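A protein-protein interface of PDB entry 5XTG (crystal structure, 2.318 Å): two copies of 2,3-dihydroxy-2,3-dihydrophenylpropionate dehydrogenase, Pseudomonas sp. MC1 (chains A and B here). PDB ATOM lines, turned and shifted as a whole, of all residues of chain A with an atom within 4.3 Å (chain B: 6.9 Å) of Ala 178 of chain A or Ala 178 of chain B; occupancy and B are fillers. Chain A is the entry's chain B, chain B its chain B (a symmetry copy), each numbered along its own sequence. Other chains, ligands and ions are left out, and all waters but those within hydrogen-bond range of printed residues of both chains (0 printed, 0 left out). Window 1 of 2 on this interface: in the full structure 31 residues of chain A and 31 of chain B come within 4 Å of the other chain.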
ATOM      1  N   VAL A 133     -32.224  -0.183   7.141  1.00  0.00           N
ATOM      2  CA  VAL A 133     -31.870  -0.502   5.763  1.00  0.00           C
ATOM      3  C   VAL A 133     -33.015  -0.141   4.832  1.00  0.00           C
ATOM      4  O   VAL A 133     -32.899   0.761   3.999  1.00  0.00           O
ATOM      5  CB  VAL A 133     -31.491  -1.980   5.638  1.00  0.00           C
ATOM      6  CG1 VAL A 133     -30.825  -2.233   4.304  1.00  0.00           C
ATOM      7  CG2 VAL A 133     -30.516  -2.379   6.760  1.00  0.00           C
ATOM      8  N   ALA A 174     -25.160  -6.790  11.165  1.00  0.00           N
ATOM      9  CA  ALA A 174     -25.552  -7.148   9.811  1.00  0.00           C
ATOM     10  C   ALA A 174     -26.248  -5.989   9.130  1.00  0.00           C
ATOM     11  O   ALA A 174     -25.992  -5.706   7.950  1.00  0.00           O
ATOM     12  CB  ALA A 174     -26.463  -8.370   9.821  1.00  0.00           C
ATOM     13  N   SER A 175     -27.138  -5.305   9.851  1.00  0.00           N
ATOM     14  CA  SER A 175     -27.882  -4.207   9.238  1.00  0.00           C
ATOM     15  C   SER A 175     -26.936  -3.103   8.822  1.00  0.00           C
ATOM     16  O   SER A 175     -27.098  -2.497   7.758  1.00  0.00           O
ATOM     17  CB  SER A 175     -28.960  -3.678  10.196  1.00  0.00           C
ATOM     18  OG  SER A 175     -28.447  -2.890  11.260  1.00  0.00           O
ATOM     19  N   LYS A 176     -25.892  -2.881   9.602  1.00  0.00           N
ATOM     20  CA  LYS A 176     -24.977  -1.797   9.267  1.00  0.00           C
ATOM     21  C   LYS A 176     -23.981  -2.203   8.197  1.00  0.00           C
ATOM     22  O   LYS A 176     -23.645  -1.388   7.330  1.00  0.00           O
ATOM     23  CB  LYS A 176     -24.302  -1.338  10.540  1.00  0.00           C
ATOM     24  CG  LYS A 176     -25.260  -0.599  11.475  1.00  0.00           C
ATOM     25  CD  LYS A 176     -25.669   0.702  10.830  1.00  0.00           C
ATOM     26  CE  LYS A 176     -26.473   1.552  11.776  1.00  0.00           C
ATOM     27  NZ  LYS A 176     -27.019   2.800  11.105  1.00  0.00           N
ATOM     28  N   HIS A 177     -23.560  -3.459   8.178  1.00  0.00           N
ATOM     29  CA  HIS A 177     -22.821  -3.936   7.014  1.00  0.00           C
ATOM     30  C   HIS A 177     -23.645  -3.759   5.745  1.00  0.00           C
ATOM     31  O   HIS A 177     -23.114  -3.412   4.680  1.00  0.00           O
ATOM     32  CB  HIS A 177     -22.431  -5.389   7.200  1.00  0.00           C
ATOM     33  CG  HIS A 177     -21.146  -5.583   7.925  1.00  0.00           C
ATOM     34  ND1 HIS A 177     -20.983  -5.244   9.249  1.00  0.00           N
ATOM     35  CD2 HIS A 177     -19.939  -6.042   7.499  1.00  0.00           C
ATOM     36  CE1 HIS A 177     -19.739  -5.520   9.623  1.00  0.00           C
ATOM     37  NE2 HIS A 177     -19.082  -5.990   8.577  1.00  0.00           N
ATOM     38  N   ALA A 178     -24.945  -3.977   5.838  1.00  0.00           N
ATOM     39  CA  ALA A 178     -25.814  -3.807   4.670  1.00  0.00           C
ATOM     40  C   ALA A 178     -25.840  -2.366   4.166  1.00  0.00           C
ATOM     41  O   ALA A 178     -25.893  -2.125   2.951  1.00  0.00           O
ATOM     42  CB  ALA A 178     -27.223  -4.249   5.032  1.00  0.00           C
ATOM     43  N   VAL A 179     -25.831  -1.390   5.084  1.00  0.00           N
ATOM     44  CA  VAL A 179     -25.697   0.021   4.700  1.00  0.00           C
ATOM     45  C   VAL A 179     -24.434   0.252   3.882  1.00  0.00           C
ATOM     46  O   VAL A 179     -24.432   1.036   2.924  1.00  0.00           O
ATOM     47  CB  VAL A 179     -25.667   0.933   5.936  1.00  0.00           C
ATOM     48  CG1 VAL A 179     -25.317   2.357   5.508  1.00  0.00           C
ATOM     49  CG2 VAL A 179     -26.983   0.932   6.657  1.00  0.00           C
ATOM     50  N   LEU A 180     -23.314  -0.334   4.307  1.00  0.00           N
ATOM     51  CA  LEU A 180     -22.082  -0.172   3.528  1.00  0.00           C
ATOM     52  C   LEU A 180     -22.294  -0.676   2.128  1.00  0.00           C
ATOM     53  O   LEU A 180     -21.819  -0.073   1.164  1.00  0.00           O
ATOM     54  CB  LEU A 180     -20.919  -0.971   4.099  1.00  0.00           C
ATOM     55  CG  LEU A 180     -20.256  -0.727   5.428  1.00  0.00           C
ATOM     56  CD1 LEU A 180     -18.909  -1.479   5.381  1.00  0.00           C
ATOM     57  CD2 LEU A 180     -20.088   0.765   5.645  1.00  0.00           C
ATOM     58  N   GLY A 181     -22.946  -1.837   2.014  1.00  0.00           N
ATOM     59  CA  GLY A 181     -23.290  -2.366   0.705  1.00  0.00           C
ATOM     60  C   GLY A 181     -24.067  -1.368  -0.110  1.00  0.00           C
ATOM     61  O   GLY A 181     -23.757  -1.139  -1.280  1.00  0.00           O
ATOM     62  N   MET A 182     -25.073  -0.734   0.515  1.00  0.00           N
ATOM     63  CA  MET A 182     -25.879   0.263  -0.190  1.00  0.00           C
ATOM     64  C   MET A 182     -25.023   1.397  -0.689  1.00  0.00           C
ATOM     65  O   MET A 182     -25.209   1.884  -1.802  1.00  0.00           O
ATOM     66  CB  MET A 182     -26.934   0.876   0.715  1.00  0.00           C
ATOM     67  CG  MET A 182     -28.015  -0.060   1.114  1.00  0.00           C
ATOM     68  SD  MET A 182     -29.178   0.801   2.199  1.00  0.00           S
ATOM     69  CE  MET A 182     -29.686   2.158   1.117  1.00  0.00           C
ATOM     70  N   PHE B 129     -34.100 -10.089   1.273  1.00  0.00           N
ATOM     71  CA  PHE B 129     -33.578 -10.024   2.630  1.00  0.00           C
ATOM     72  C   PHE B 129     -34.146 -11.121   3.499  1.00  0.00           C
ATOM     73  O   PHE B 129     -33.447 -11.593   4.398  1.00  0.00           O
ATOM     74  CB  PHE B 129     -33.847  -8.650   3.232  1.00  0.00           C
ATOM     75  CG  PHE B 129     -32.730  -7.668   2.978  1.00  0.00           C
ATOM     76  CD1 PHE B 129     -32.616  -7.032   1.759  1.00  0.00           C
ATOM     77  CD2 PHE B 129     -31.765  -7.430   3.943  1.00  0.00           C
ATOM     78  CE1 PHE B 129     -31.575  -6.155   1.509  1.00  0.00           C
ATOM     79  CE2 PHE B 129     -30.710  -6.548   3.698  1.00  0.00           C
ATOM     80  CZ  PHE B 129     -30.621  -5.915   2.480  1.00  0.00           C
ATOM     81  N   ASN B 132     -31.931 -14.265   1.784  1.00  0.00           N
ATOM     82  CA  ASN B 132     -30.476 -14.162   1.858  1.00  0.00           C
ATOM     83  C   ASN B 132     -29.935 -13.793   3.232  1.00  0.00           C
ATOM     84  O   ASN B 132     -28.717 -13.851   3.424  1.00  0.00           O
ATOM     85  CB  ASN B 132     -29.964 -13.094   0.901  1.00  0.00           C
ATOM     86  CG  ASN B 132     -30.250 -13.412  -0.509  1.00  0.00           C
ATOM     87  OD1 ASN B 132     -30.828 -14.458  -0.822  1.00  0.00           O
ATOM     88  ND2 ASN B 132     -29.889 -12.496  -1.387  1.00  0.00           N
ATOM     89  N   VAL B 133     -30.769 -13.332   4.161  1.00  0.00           N
ATOM     90  CA  VAL B 133     -30.271 -12.902   5.462  1.00  0.00           C
ATOM     91  C   VAL B 133     -31.102 -13.521   6.572  1.00  0.00           C
ATOM     92  O   VAL B 133     -30.614 -14.344   7.350  1.00  0.00           O
ATOM     93  CB  VAL B 133     -30.267 -11.373   5.553  1.00  0.00           C
ATOM     94  CG1 VAL B 133     -29.463 -10.927   6.754  1.00  0.00           C
ATOM     95  CG2 VAL B 133     -29.641 -10.764   4.285  1.00  0.00           C
ATOM     96  N   PHE B 137     -30.220 -16.427   9.665  1.00  0.00           N
ATOM     97  CA  PHE B 137     -30.424 -16.307  11.107  1.00  0.00           C
ATOM     98  C   PHE B 137     -31.282 -17.451  11.609  1.00  0.00           C
ATOM     99  O   PHE B 137     -30.954 -18.089  12.621  1.00  0.00           O
ATOM    100  CB  PHE B 137     -31.088 -14.982  11.439  1.00  0.00           C
ATOM    101  CG  PHE B 137     -30.136 -13.838  11.547  1.00  0.00           C
ATOM    102  CD1 PHE B 137     -29.896 -13.010  10.456  1.00  0.00           C
ATOM    103  CD2 PHE B 137     -29.478 -13.575  12.726  1.00  0.00           C
ATOM    104  CE1 PHE B 137     -29.001 -11.943  10.537  1.00  0.00           C
ATOM    105  CE2 PHE B 137     -28.577 -12.499  12.817  1.00  0.00           C
ATOM    106  CZ  PHE B 137     -28.356 -11.687  11.728  1.00  0.00           C
ATOM    107  N   SER B 162     -20.633  -9.423  -1.751  1.00  0.00           N
ATOM    108  CA  SER B 162     -20.277  -9.054  -0.392  1.00  0.00           C
ATOM    109  C   SER B 162     -19.100  -8.096  -0.310  1.00  0.00           C
ATOM    110  O   SER B 162     -18.907  -7.492   0.749  1.00  0.00           O
ATOM    111  CB  SER B 162     -19.925 -10.289   0.408  1.00  0.00           C
ATOM    112  OG  SER B 162     -21.064 -11.118   0.576  1.00  0.00           O
ATOM    113  N   SER B 170     -28.539  -2.934  -5.923  1.00  0.00           N
ATOM    114  CA  SER B 170     -28.239  -2.506  -4.563  1.00  0.00           C
ATOM    115  C   SER B 170     -28.876  -3.413  -3.512  1.00  0.00           C
ATOM    116  O   SER B 170     -28.302  -3.587  -2.432  1.00  0.00           O
ATOM    117  CB  SER B 170     -28.689  -1.076  -4.378  1.00  0.00           C
ATOM    118  OG  SER B 170     -30.060  -0.960  -4.704  1.00  0.00           O
ATOM    119  N   TYR B 172     -29.368  -6.749  -3.746  1.00  0.00           N
ATOM    120  CA  TYR B 172     -28.582  -7.976  -3.628  1.00  0.00           C
ATOM    121  C   TYR B 172     -27.283  -7.714  -2.888  1.00  0.00           C
ATOM    122  O   TYR B 172     -26.926  -8.440  -1.954  1.00  0.00           O
ATOM    123  CB  TYR B 172     -28.297  -8.562  -5.009  1.00  0.00           C
ATOM    124  CG  TYR B 172     -27.579  -9.878  -4.953  1.00  0.00           C
ATOM    125  CD1 TYR B 172     -28.250 -11.041  -4.550  1.00  0.00           C
ATOM    126  CD2 TYR B 172     -26.231  -9.969  -5.289  1.00  0.00           C
ATOM    127  CE1 TYR B 172     -27.598 -12.260  -4.486  1.00  0.00           C
ATOM    128  CE2 TYR B 172     -25.560 -11.190  -5.233  1.00  0.00           C
ATOM    129  CZ  TYR B 172     -26.256 -12.330  -4.820  1.00  0.00           C
ATOM    130  OH  TYR B 172     -25.609 -13.540  -4.753  1.00  0.00           O
ATOM    131  N   ILE B 173     -26.567  -6.663  -3.305  1.00  0.00           N
ATOM    132  CA  ILE B 173     -25.287  -6.307  -2.722  1.00  0.00           C
ATOM    133  C   ILE B 173     -25.439  -5.995  -1.240  1.00  0.00           C
ATOM    134  O   ILE B 173     -24.639  -6.423  -0.400  1.00  0.00           O
ATOM    135  CB  ILE B 173     -24.701  -5.121  -3.502  1.00  0.00           C
ATOM    136  CG1 ILE B 173     -24.273  -5.593  -4.902  1.00  0.00           C
ATOM    137  CG2 ILE B 173     -23.541  -4.543  -2.753  1.00  0.00           C
ATOM    138  CD1 ILE B 173     -23.904  -4.497  -5.913  1.00  0.00           C
ATOM    139  N   ALA B 174     -26.456  -5.233  -0.893  1.00  0.00           N
ATOM    140  CA  ALA B 174     -26.681  -4.955   0.517  1.00  0.00           C
ATOM    141  C   ALA B 174     -26.925  -6.238   1.283  1.00  0.00           C
ATOM    142  O   ALA B 174     -26.401  -6.419   2.392  1.00  0.00           O
ATOM    143  CB  ALA B 174     -27.861  -4.008   0.696  1.00  0.00           C
ATOM    144  N   SER B 175     -27.724  -7.143   0.715  1.00  0.00           N
ATOM    145  CA  SER B 175     -28.042  -8.381   1.424  1.00  0.00           C
ATOM    146  C   SER B 175     -26.786  -9.196   1.641  1.00  0.00           C
ATOM    147  O   SER B 175     -26.598  -9.799   2.702  1.00  0.00           O
ATOM    148  CB  SER B 175     -29.101  -9.190   0.659  1.00  0.00           C
ATOM    149  OG  SER B 175     -28.599  -9.845  -0.497  1.00  0.00           O
ATOM    150  N   LYS B 176     -25.876  -9.162   0.684  1.00  0.00           N
ATOM    151  CA  LYS B 176     -24.670  -9.968   0.827  1.00  0.00           C
ATOM    152  C   LYS B 176     -23.638  -9.295   1.713  1.00  0.00           C
ATOM    153  O   LYS B 176     -22.957  -9.977   2.488  1.00  0.00           O
ATOM    154  CB  LYS B 176     -24.135 -10.267  -0.556  1.00  0.00           C
ATOM    155  CG  LYS B 176     -25.022 -11.249  -1.324  1.00  0.00           C
ATOM    156  CD  LYS B 176     -24.964 -12.596  -0.647  1.00  0.00           C
ATOM    157  CE  LYS B 176     -25.678 -13.645  -1.456  1.00  0.00           C
ATOM    158  NZ  LYS B 176     -25.759 -14.975  -0.727  1.00  0.00           N
ATOM    159  N   HIS B 177     -23.556  -7.973   1.687  1.00  0.00           N
ATOM    160  CA  HIS B 177     -22.770  -7.297   2.713  1.00  0.00           C
ATOM    161  C   HIS B 177     -23.283  -7.649   4.102  1.00  0.00           C
ATOM    162  O   HIS B 177     -22.502  -7.824   5.049  1.00  0.00           O
ATOM    163  CB  HIS B 177     -22.804  -5.797   2.494  1.00  0.00           C
ATOM    164  CG  HIS B 177     -21.760  -5.297   1.558  1.00  0.00           C
ATOM    165  ND1 HIS B 177     -21.752  -5.614   0.219  1.00  0.00           N
ATOM    166  CD2 HIS B 177     -20.655  -4.535   1.775  1.00  0.00           C
ATOM    167  CE1 HIS B 177     -20.706  -5.038  -0.362  1.00  0.00           C
ATOM    168  NE2 HIS B 177     -20.017  -4.391   0.562  1.00  0.00           N
ATOM    169  N   ALA B 178     -24.592  -7.773   4.245  1.00  0.00           N
ATOM    170  CA  ALA B 178     -25.167  -8.132   5.544  1.00  0.00           C
ATOM    171  C   ALA B 178     -24.734  -9.520   6.012  1.00  0.00           C
ATOM    172  O   ALA B 178     -24.509  -9.738   7.211  1.00  0.00           O
ATOM    173  CB  ALA B 178     -26.684  -8.074   5.448  1.00  0.00           C
ATOM    174  N   VAL B 179     -24.638 -10.483   5.084  1.00  0.00           N
ATOM    175  CA  VAL B 179     -24.083 -11.803   5.406  1.00  0.00           C
ATOM    176  C   VAL B 179     -22.678 -11.684   5.982  1.00  0.00           C
ATOM    177  O   VAL B 179     -22.306 -12.419   6.907  1.00  0.00           O
ATOM    178  CB  VAL B 179     -24.039 -12.705   4.163  1.00  0.00           C
ATOM    179  CG1 VAL B 179     -23.266 -13.982   4.489  1.00  0.00           C
ATOM    180  CG2 VAL B 179     -25.417 -13.057   3.686  1.00  0.00           C
ATOM    181  N   LEU B 180     -21.839 -10.841   5.380  1.00  0.00           N
ATOM    182  CA  LEU B 180     -20.489 -10.664   5.925  1.00  0.00           C
ATOM    183  C   LEU B 180     -20.571 -10.199   7.352  1.00  0.00           C
ATOM    184  O   LEU B 180     -19.796 -10.638   8.203  1.00  0.00           O
ATOM    185  CB  LEU B 180     -19.689  -9.608   5.176  1.00  0.00           C
ATOM    186  CG  LEU B 180     -19.231  -9.705   3.745  1.00  0.00           C
ATOM    187  CD1 LEU B 180     -18.135  -8.633   3.572  1.00  0.00           C
ATOM    188  CD2 LEU B 180     -18.728 -11.109   3.468  1.00  0.00           C
ATOM    189  N   GLY B 181     -21.469  -9.241   7.606  1.00  0.00           N
ATOM    190  CA  GLY B 181     -21.700  -8.788   8.967  1.00  0.00           C
ATOM    191  C   GLY B 181     -22.039  -9.932   9.883  1.00  0.00           C
ATOM    192  O   GLY B 181     -21.480 -10.047  10.974  1.00  0.00           O
ATOM    193  N   MET B 182     -22.943 -10.816   9.431  1.00  0.00           N
ATOM    194  CA  MET B 182     -23.330 -11.970  10.244  1.00  0.00           C
ATOM    195  C   MET B 182     -22.138 -12.835  10.557  1.00  0.00           C
ATOM    196  O   MET B 182     -21.994 -13.327  11.674  1.00  0.00           O
ATOM    197  CB  MET B 182     -24.335 -12.853   9.525  1.00  0.00           C
ATOM    198  CG  MET B 182     -25.673 -12.234   9.346  1.00  0.00           C
ATOM    199  SD  MET B 182     -26.750 -13.389   8.463  1.00  0.00           S
ATOM    200  CE  MET B 182     -26.694 -14.806   9.586  1.00  0.00           C
ATOM    201  N   VAL B 183     -21.322 -13.114   9.547  1.00  0.00           N
ATOM    202  CA  VAL B 183     -20.144 -13.957   9.766  1.00  0.00           C
ATOM    203  C   VAL B 183     -19.261 -13.374  10.868  1.00  0.00           C
ATOM    204  O   VAL B 183     -18.914 -14.057  11.830  1.00  0.00           O
ATOM    205  CB  VAL B 183     -19.356 -14.128   8.457  1.00  0.00           C
ATOM    206  CG1 VAL B 183     -18.089 -14.835   8.722  1.00  0.00           C
ATOM    207  CG2 VAL B 183     -20.181 -14.905   7.496  1.00  0.00           C
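A ring nitrogen (NE2) of His 177 of chain B lies close to the backbone carbonyl oxygen (O) of Ser 162 of chain B, at 3.3 Å. O of Ile 173 of chain B lies within hydrogen-bond range of ND1 of His 177 of chain B (3.1 Å).
Ala 174 of chain A touches Ala 178 of chain B (O to CB, 3.5 Å). Met 182 of chain B touches Ala 174 of chain A (CG to CB, 3.97 Å). CB of His 177 of chain A touches O of His 177 of chain B, 3.2 Å away. His 177 of chain A touches Gly 181 of chain B. CB of Ala 178 of chain A touches O of Ala 174 of chain B, 3.5 Å away. Ala 178 of chain B touches Ala 178 of chain A (CB to CB, 3.9 Å). Gly 181 of chain A touches Ile 173 of chain B (O to CG2, 3.7 Å). His 177 of chain B touches Gly 181 of chain A. CB of Ala 174 of chain B touches CG of Met 182 of chain A (3.97 Å).
Of the printed residues of chain B, Ala 174 of chain A touches Ala 178 and Met 182. Of the printed residues of chain B, His 177 of chain A touches His 177 (3.2 Å) and Gly 181 (3.4 Å). Of chain B, only Ala 174 and Ala 178 come within 4 Å of Ala 178 of chain A. Of the printed residues of chain B, Met 182 of chain A touches Ala 174. Ser 170 of chain B touches none of the printed residues of chain A. Tyr 172 of chain B touches none of the printed residues of chain A. Printed residues of chain A within 4 Å of Ala 174 of chain B: Ala 178 (3.5 Å) and Met 182 (3.97 Å). Ala 178 of chain B touches just these residues of chain A: Ala 174 (3.5 Å) and Ala 178 (3.9 Å). The nearest residue of chain B that does not touch Ala 178 of chain A is His 177 of chain B (4.2 Å). The nearest printed residue of chain B that does not touch Gly 181 of chain A is Ala 174 of chain B (4.3 Å).
Of the 10 printed residues of chain A, 5 touch a printed residue of chain B. Hydrophobic or aromatic side chains of chain A that line the printed part of chain B: Ala 174, His 177, Ala 178 and Met 182. Of the 18 printed residues of chain B, 6 touch a printed residue of chain A.
Ala 174 of chain A touches Ala 178 of chain B, and with the chains exchanged Ala 178 of chain A touches Ala 174 of chain B. His 177 of chain A touches its own counterpart, His 177 of chain B. His 177 of chain A touches Gly 181 of chain B, and with the chains exchanged Gly 181 of chain A touches His 177 of chain B. Ala 178 of chain A touches its own counterpart, Ala 178 of chain B. Positions printed for both chains: 133, 174, 175, 176, 177, 178, 179, 180, 181 and 182. Of the 9 pairs that touch across the chains among the printed residues, 8 have their exchanged pair printed and touching as well.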
